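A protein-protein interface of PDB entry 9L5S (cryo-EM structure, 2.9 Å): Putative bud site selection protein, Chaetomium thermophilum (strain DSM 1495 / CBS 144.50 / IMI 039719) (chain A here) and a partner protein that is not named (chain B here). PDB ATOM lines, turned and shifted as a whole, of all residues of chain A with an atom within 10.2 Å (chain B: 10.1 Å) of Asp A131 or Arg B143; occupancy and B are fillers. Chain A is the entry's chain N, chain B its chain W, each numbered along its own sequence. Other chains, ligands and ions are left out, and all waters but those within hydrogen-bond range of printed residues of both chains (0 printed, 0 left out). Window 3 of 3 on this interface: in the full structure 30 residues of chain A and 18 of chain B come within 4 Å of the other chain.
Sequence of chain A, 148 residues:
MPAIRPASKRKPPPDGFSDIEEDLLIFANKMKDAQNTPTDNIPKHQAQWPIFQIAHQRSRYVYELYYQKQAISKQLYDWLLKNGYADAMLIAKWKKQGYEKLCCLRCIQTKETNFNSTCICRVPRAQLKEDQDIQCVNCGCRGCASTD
The backbone carbonyl oxygen (O) of Lys A129 lies within hydrogen-bond range of the guanidinium group (NH1) of Arg A125 (2.6 Å). N of Lys A129 sits at hydrogen-bond distance from OE1 of Gln A132 (3.0 Å).
CG of Arg A125 touches CD2 of Leu B115, 3.7 Å away. Tyr B141 touches Arg A125 (OH to CB, 3.5 Å). CG2 of Val B97 touches O of Leu A128 (3.4 Å). Lys A129 touches Val B97. Arg B143 touches Asp A131 (CD to OD1, 3.3 Å).
Asp A131 touches just one residue of chain B: Arg B143 (3.3 Å). Arg B143 touches one residue of chain A. Glu A130 touches none of the printed residues of chain B. Of the printed residues of chain A, Tyr B141 touches Arg A125 (3.5 Å). Of the printed residues of chain A, Val B97 touches Leu A128 (3.4 Å) and Lys A129 (3.8 Å). Of the printed residues of chain A, Leu B115 touches Arg A125 (3.7 Å). Of the printed residues of chain B, Lys A129 touches Val B97 (3.8 Å). Of the printed residues of chain B, Arg A125 touches Leu B115 and Tyr B141.
Along chain A the printed residues that touch a printed residue of chain B span positions 125 to 131. Hydrophobic or aromatic side chains of chain B that line the printed part of chain A: Val B97, Leu B115 and Tyr B141. Among the printed residues, no Asp or Glu carboxylate lies within 4 Å of a Lys or Arg side-chain nitrogen of the other chain.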
ATOM      1  N   ARG A 125      -1.584   9.353  34.093  1.00  0.00           N
ATOM      2  CA  ARG A 125      -0.988   8.285  33.299  1.00  0.00           C
ATOM      3  C   ARG A 125      -0.247   7.270  34.167  1.00  0.00           C
ATOM      4  O   ARG A 125      -0.101   6.110  33.762  1.00  0.00           O
ATOM      5  CB  ARG A 125      -0.058   8.911  32.250  1.00  0.00           C
ATOM      6  CG  ARG A 125       0.672   7.949  31.328  1.00  0.00           C
ATOM      7  CD  ARG A 125      -0.315   7.220  30.431  1.00  0.00           C
ATOM      8  NE  ARG A 125       0.349   6.310  29.506  1.00  0.00           N
ATOM      9  CZ  ARG A 125       0.677   5.058  29.792  1.00  0.00           C
ATOM     10  NH1 ARG A 125       0.411   4.526  30.974  1.00  0.00           N
ATOM     11  NH2 ARG A 125       1.284   4.319  28.868  1.00  0.00           N
ATOM     12  N   LEU A 128      -2.294   4.220  35.025  1.00  0.00           N
ATOM     13  CA  LEU A 128      -2.670   3.413  33.877  1.00  0.00           C
ATOM     14  C   LEU A 128      -1.517   2.494  33.497  1.00  0.00           C
ATOM     15  O   LEU A 128      -0.365   2.719  33.876  1.00  0.00           O
ATOM     16  CB  LEU A 128      -3.057   4.299  32.687  1.00  0.00           C
ATOM     17  CG  LEU A 128      -4.418   4.994  32.776  1.00  0.00           C
ATOM     18  CD1 LEU A 128      -4.692   5.798  31.518  1.00  0.00           C
ATOM     19  CD2 LEU A 128      -5.527   3.985  33.023  1.00  0.00           C
ATOM     20  N   LYS A 129      -1.846   1.440  32.756  1.00  0.00           N
ATOM     21  CA  LYS A 129      -0.859   0.443  32.370  1.00  0.00           C
ATOM     22  C   LYS A 129       0.131   1.015  31.359  1.00  0.00           C
ATOM     23  O   LYS A 129      -0.125   2.023  30.694  1.00  0.00           O
ATOM     24  CB  LYS A 129      -1.545  -0.782  31.766  1.00  0.00           C
ATOM     25  CG  LYS A 129      -2.147  -1.742  32.774  1.00  0.00           C
ATOM     26  CD  LYS A 129      -1.958  -3.185  32.326  1.00  0.00           C
ATOM     27  CE  LYS A 129      -2.506  -3.397  30.918  1.00  0.00           C
ATOM     28  NZ  LYS A 129      -2.310  -4.789  30.428  1.00  0.00           N
ATOM     29  N   GLU A 130       1.280   0.356  31.254  1.00  0.00           N
ATOM     30  CA  GLU A 130       2.195   0.648  30.164  1.00  0.00           C
ATOM     31  C   GLU A 130       1.695  -0.014  28.884  1.00  0.00           C
ATOM     32  O   GLU A 130       0.920  -0.976  28.917  1.00  0.00           O
ATOM     33  CB  GLU A 130       3.609   0.173  30.497  1.00  0.00           C
ATOM     34  CG  GLU A 130       4.217   0.854  31.714  1.00  0.00           C
ATOM     35  CD  GLU A 130       4.374   2.352  31.529  1.00  0.00           C
ATOM     36  OE1 GLU A 130       4.720   2.784  30.408  1.00  0.00           O
ATOM     37  OE2 GLU A 130       4.144   3.099  32.503  1.00  0.00           O
ATOM     38  N   ASP A 131       2.135   0.536  27.748  1.00  0.00           N
ATOM     39  CA  ASP A 131       1.652   0.190  26.407  1.00  0.00           C
ATOM     40  C   ASP A 131       0.140   0.348  26.268  1.00  0.00           C
ATOM     41  O   ASP A 131      -0.478  -0.295  25.412  1.00  0.00           O
ATOM     42  CB  ASP A 131       2.073  -1.227  25.991  1.00  0.00           C
ATOM     43  CG  ASP A 131       3.556  -1.336  25.711  1.00  0.00           C
ATOM     44  OD1 ASP A 131       4.156  -0.321  25.302  1.00  0.00           O
ATOM     45  OD2 ASP A 131       4.120  -2.437  25.887  1.00  0.00           O
ATOM     46  N   GLN A 132      -0.474   1.192  27.096  1.00  0.00           N
ATOM     47  CA  GLN A 132      -1.907   1.463  27.036  1.00  0.00           C
ATOM     48  C   GLN A 132      -2.091   2.846  26.424  1.00  0.00           C
ATOM     49  O   GLN A 132      -2.144   3.855  27.126  1.00  0.00           O
ATOM     50  CB  GLN A 132      -2.547   1.382  28.415  1.00  0.00           C
ATOM     51  CG  GLN A 132      -4.061   1.344  28.362  1.00  0.00           C
ATOM     52  CD  GLN A 132      -4.699   1.247  29.730  1.00  0.00           C
ATOM     53  OE1 GLN A 132      -4.022   1.027  30.730  1.00  0.00           O
ATOM     54  NE2 GLN A 132      -6.010   1.432  29.781  1.00  0.00           N
ATOM     55  N   ASP A 133      -2.184   2.891  25.098  1.00  0.00           N
ATOM     56  CA  ASP A 133      -2.479   4.141  24.405  1.00  0.00           C
ATOM     57  C   ASP A 133      -3.993   4.267  24.346  1.00  0.00           C
ATOM     58  O   ASP A 133      -4.635   3.873  23.371  1.00  0.00           O
ATOM     59  CB  ASP A 133      -1.848   4.166  23.019  1.00  0.00           C
ATOM     60  CG  ASP A 133      -2.092   5.478  22.297  1.00  0.00           C
ATOM     61  OD1 ASP A 133      -3.072   5.566  21.529  1.00  0.00           O
ATOM     62  OD2 ASP A 133      -1.302   6.424  22.503  1.00  0.00           O
ATOM     63  N   ILE A 134      -4.574   4.805  25.420  1.00  0.00           N
ATOM     64  CA  ILE A 134      -6.004   5.070  25.431  1.00  0.00           C
ATOM     65  C   ILE A 134      -6.312   6.199  24.457  1.00  0.00           C
ATOM     66  O   ILE A 134      -5.476   7.073  24.191  1.00  0.00           O
ATOM     67  CB  ILE A 134      -6.503   5.406  26.851  1.00  0.00           C
ATOM     68  CG1 ILE A 134      -5.894   6.717  27.352  1.00  0.00           C
ATOM     69  CG2 ILE A 134      -6.203   4.269  27.810  1.00  0.00           C
ATOM     70  CD1 ILE A 134      -6.625   7.323  28.526  1.00  0.00           C
ATOM     71  N   GLN A 135      -7.513   6.165  23.894  1.00  0.00           N
ATOM     72  CA  GLN A 135      -7.918   7.201  22.951  1.00  0.00           C
ATOM     73  C   GLN A 135      -9.422   7.375  23.136  1.00  0.00           C
ATOM     74  O   GLN A 135     -10.209   6.546  22.670  1.00  0.00           O
ATOM     75  CB  GLN A 135      -7.531   6.831  21.526  1.00  0.00           C
ATOM     76  CG  GLN A 135      -7.517   8.001  20.560  1.00  0.00           C
ATOM     77  CD  GLN A 135      -6.956   7.620  19.204  1.00  0.00           C
ATOM     78  OE1 GLN A 135      -6.671   6.452  18.944  1.00  0.00           O
ATOM     79  NE2 GLN A 135      -6.763   8.611  18.345  1.00  0.00           N
ATOM     80  N   VAL B  97      -3.008   0.427  38.720  1.00  0.00           N
ATOM     81  CA  VAL B  97      -1.670  -0.152  38.800  1.00  0.00           C
ATOM     82  C   VAL B  97      -0.801   0.805  39.618  1.00  0.00           C
ATOM     83  O   VAL B  97      -0.325   1.842  39.150  1.00  0.00           O
ATOM     84  CB  VAL B  97      -1.095  -0.485  37.417  1.00  0.00           C
ATOM     85  CG1 VAL B  97      -1.924  -1.587  36.794  1.00  0.00           C
ATOM     86  CG2 VAL B  97      -1.192   0.686  36.452  1.00  0.00           C
ATOM     87  N   LEU B 115       7.058  10.517  32.882  1.00  0.00           N
ATOM     88  CA  LEU B 115       5.954  10.178  31.988  1.00  0.00           C
ATOM     89  C   LEU B 115       5.634  11.331  31.044  1.00  0.00           C
ATOM     90  O   LEU B 115       5.308  11.112  29.872  1.00  0.00           O
ATOM     91  CB  LEU B 115       4.722   9.788  32.802  1.00  0.00           C
ATOM     92  CG  LEU B 115       4.712   8.349  33.317  1.00  0.00           C
ATOM     93  CD1 LEU B 115       3.817   8.241  34.526  1.00  0.00           C
ATOM     94  CD2 LEU B 115       4.260   7.387  32.238  1.00  0.00           C
ATOM     95  N   MET B 118       8.339  11.593  28.364  1.00  0.00           N
ATOM     96  CA  MET B 118       8.254  10.538  27.359  1.00  0.00           C
ATOM     97  C   MET B 118       7.316  10.934  26.221  1.00  0.00           C
ATOM     98  O   MET B 118       7.573  10.601  25.058  1.00  0.00           O
ATOM     99  CB  MET B 118       7.797   9.227  28.007  1.00  0.00           C
ATOM    100  CG  MET B 118       7.476   8.107  27.022  1.00  0.00           C
ATOM    101  SD  MET B 118       7.154   6.519  27.809  1.00  0.00           S
ATOM    102  CE  MET B 118       5.856   6.980  28.947  1.00  0.00           C
ATOM    103  N   ARG B 119       6.257  11.678  26.532  1.00  0.00           N
ATOM    104  CA  ARG B 119       5.238  12.094  25.580  1.00  0.00           C
ATOM    105  C   ARG B 119       5.802  13.109  24.583  1.00  0.00           C
ATOM    106  O   ARG B 119       6.877  13.684  24.776  1.00  0.00           O
ATOM    107  CB  ARG B 119       4.047  12.693  26.328  1.00  0.00           C
ATOM    108  CG  ARG B 119       2.688  12.496  25.679  1.00  0.00           C
ATOM    109  CD  ARG B 119       1.654  13.368  26.368  1.00  0.00           C
ATOM    110  NE  ARG B 119       0.294  13.078  25.931  1.00  0.00           N
ATOM    111  CZ  ARG B 119      -0.794  13.481  26.570  1.00  0.00           C
ATOM    112  NH1 ARG B 119      -0.717  14.203  27.675  1.00  0.00           N
ATOM    113  NH2 ARG B 119      -1.989  13.151  26.091  1.00  0.00           N
ATOM    114  N   GLU B 120       5.053  13.328  23.502  1.00  0.00           N
ATOM    115  CA  GLU B 120       5.402  14.338  22.514  1.00  0.00           C
ATOM    116  C   GLU B 120       5.280  15.744  23.104  1.00  0.00           C
ATOM    117  O   GLU B 120       4.731  15.955  24.188  1.00  0.00           O
ATOM    118  CB  GLU B 120       4.501  14.231  21.284  1.00  0.00           C
ATOM    119  CG  GLU B 120       4.371  12.844  20.691  1.00  0.00           C
ATOM    120  CD  GLU B 120       3.767  12.868  19.302  1.00  0.00           C
ATOM    121  OE1 GLU B 120       2.899  13.731  19.044  1.00  0.00           O
ATOM    122  OE2 GLU B 120       4.157  12.028  18.466  1.00  0.00           O
ATOM    123  N   ALA B 139      -1.686  14.633  22.196  1.00  0.00           N
ATOM    124  CA  ALA B 139      -0.322  14.161  22.018  1.00  0.00           C
ATOM    125  C   ALA B 139      -0.204  12.720  22.494  1.00  0.00           C
ATOM    126  O   ALA B 139      -0.619  12.378  23.603  1.00  0.00           O
ATOM    127  CB  ALA B 139       0.656  15.052  22.781  1.00  0.00           C
ATOM    128  N   ARG B 140       0.367  11.877  21.645  1.00  0.00           N
ATOM    129  CA  ARG B 140       0.465  10.453  21.919  1.00  0.00           C
ATOM    130  C   ARG B 140       1.754  10.136  22.667  1.00  0.00           C
ATOM    131  O   ARG B 140       2.695  10.930  22.701  1.00  0.00           O
ATOM    132  CB  ARG B 140       0.383   9.662  20.614  1.00  0.00           C
ATOM    133  CG  ARG B 140       1.606   9.790  19.728  1.00  0.00           C
ATOM    134  CD  ARG B 140       1.227   9.634  18.265  1.00  0.00           C
ATOM    135  NE  ARG B 140       0.351  10.714  17.827  1.00  0.00           N
ATOM    136  CZ  ARG B 140      -0.297  10.736  16.671  1.00  0.00           C
ATOM    137  NH1 ARG B 140      -0.190   9.747  15.799  1.00  0.00           N
ATOM    138  NH2 ARG B 140      -1.073  11.777  16.381  1.00  0.00           N
ATOM    139  N   TYR B 141       1.776   8.964  23.292  1.00  0.00           N
ATOM    140  CA  TYR B 141       2.935   8.520  24.050  1.00  0.00           C
ATOM    141  C   TYR B 141       3.840   7.699  23.143  1.00  0.00           C
ATOM    142  O   TYR B 141       3.362   6.847  22.387  1.00  0.00           O
ATOM    143  CB  TYR B 141       2.503   7.709  25.270  1.00  0.00           C
ATOM    144  CG  TYR B 141       2.043   8.573  26.422  1.00  0.00           C
ATOM    145  CD1 TYR B 141       2.936   9.008  27.393  1.00  0.00           C
ATOM    146  CD2 TYR B 141       0.716   8.968  26.527  1.00  0.00           C
ATOM    147  CE1 TYR B 141       2.518   9.805  28.441  1.00  0.00           C
ATOM    148  CE2 TYR B 141       0.289   9.764  27.571  1.00  0.00           C
ATOM    149  CZ  TYR B 141       1.192  10.179  28.525  1.00  0.00           C
ATOM    150  OH  TYR B 141       0.771  10.972  29.566  1.00  0.00           O
ATOM    151  N   LYS B 142       5.141   7.972  23.210  1.00  0.00           N
ATOM    152  CA  LYS B 142       6.091   7.344  22.302  1.00  0.00           C
ATOM    153  C   LYS B 142       6.254   5.864  22.624  1.00  0.00           C
ATOM    154  O   LYS B 142       6.542   5.495  23.767  1.00  0.00           O
ATOM    155  CB  LYS B 142       7.446   8.045  22.387  1.00  0.00           C
ATOM    156  CG  LYS B 142       7.457   9.473  21.871  1.00  0.00           C
ATOM    157  CD  LYS B 142       8.859  10.058  21.949  1.00  0.00           C
ATOM    158  CE  LYS B 142       8.883  11.513  21.515  1.00  0.00           C
ATOM    159  NZ  LYS B 142       8.589  11.668  20.064  1.00  0.00           N
ATOM    160  N   ARG B 143       6.084   5.025  21.606  1.00  0.00           N
ATOM    161  CA  ARG B 143       6.347   3.592  21.709  1.00  0.00           C
ATOM    162  C   ARG B 143       6.488   2.974  20.324  1.00  0.00           C
ATOM    163  O   ARG B 143       5.511   2.859  19.584  1.00  0.00           O
ATOM    164  CB  ARG B 143       5.240   2.875  22.487  1.00  0.00           C
ATOM    165  CG  ARG B 143       5.419   1.359  22.607  1.00  0.00           C
ATOM    166  CD  ARG B 143       6.573   0.964  23.537  1.00  0.00           C
ATOM    167  NE  ARG B 143       7.870   0.930  22.868  1.00  0.00           N
ATOM    168  CZ  ARG B 143       9.030   0.773  23.489  1.00  0.00           C
ATOM    169  NH1 ARG B 143       9.097   0.631  24.802  1.00  0.00           N
ATOM    170  NH2 ARG B 143      10.151   0.759  22.774  1.00  0.00           N
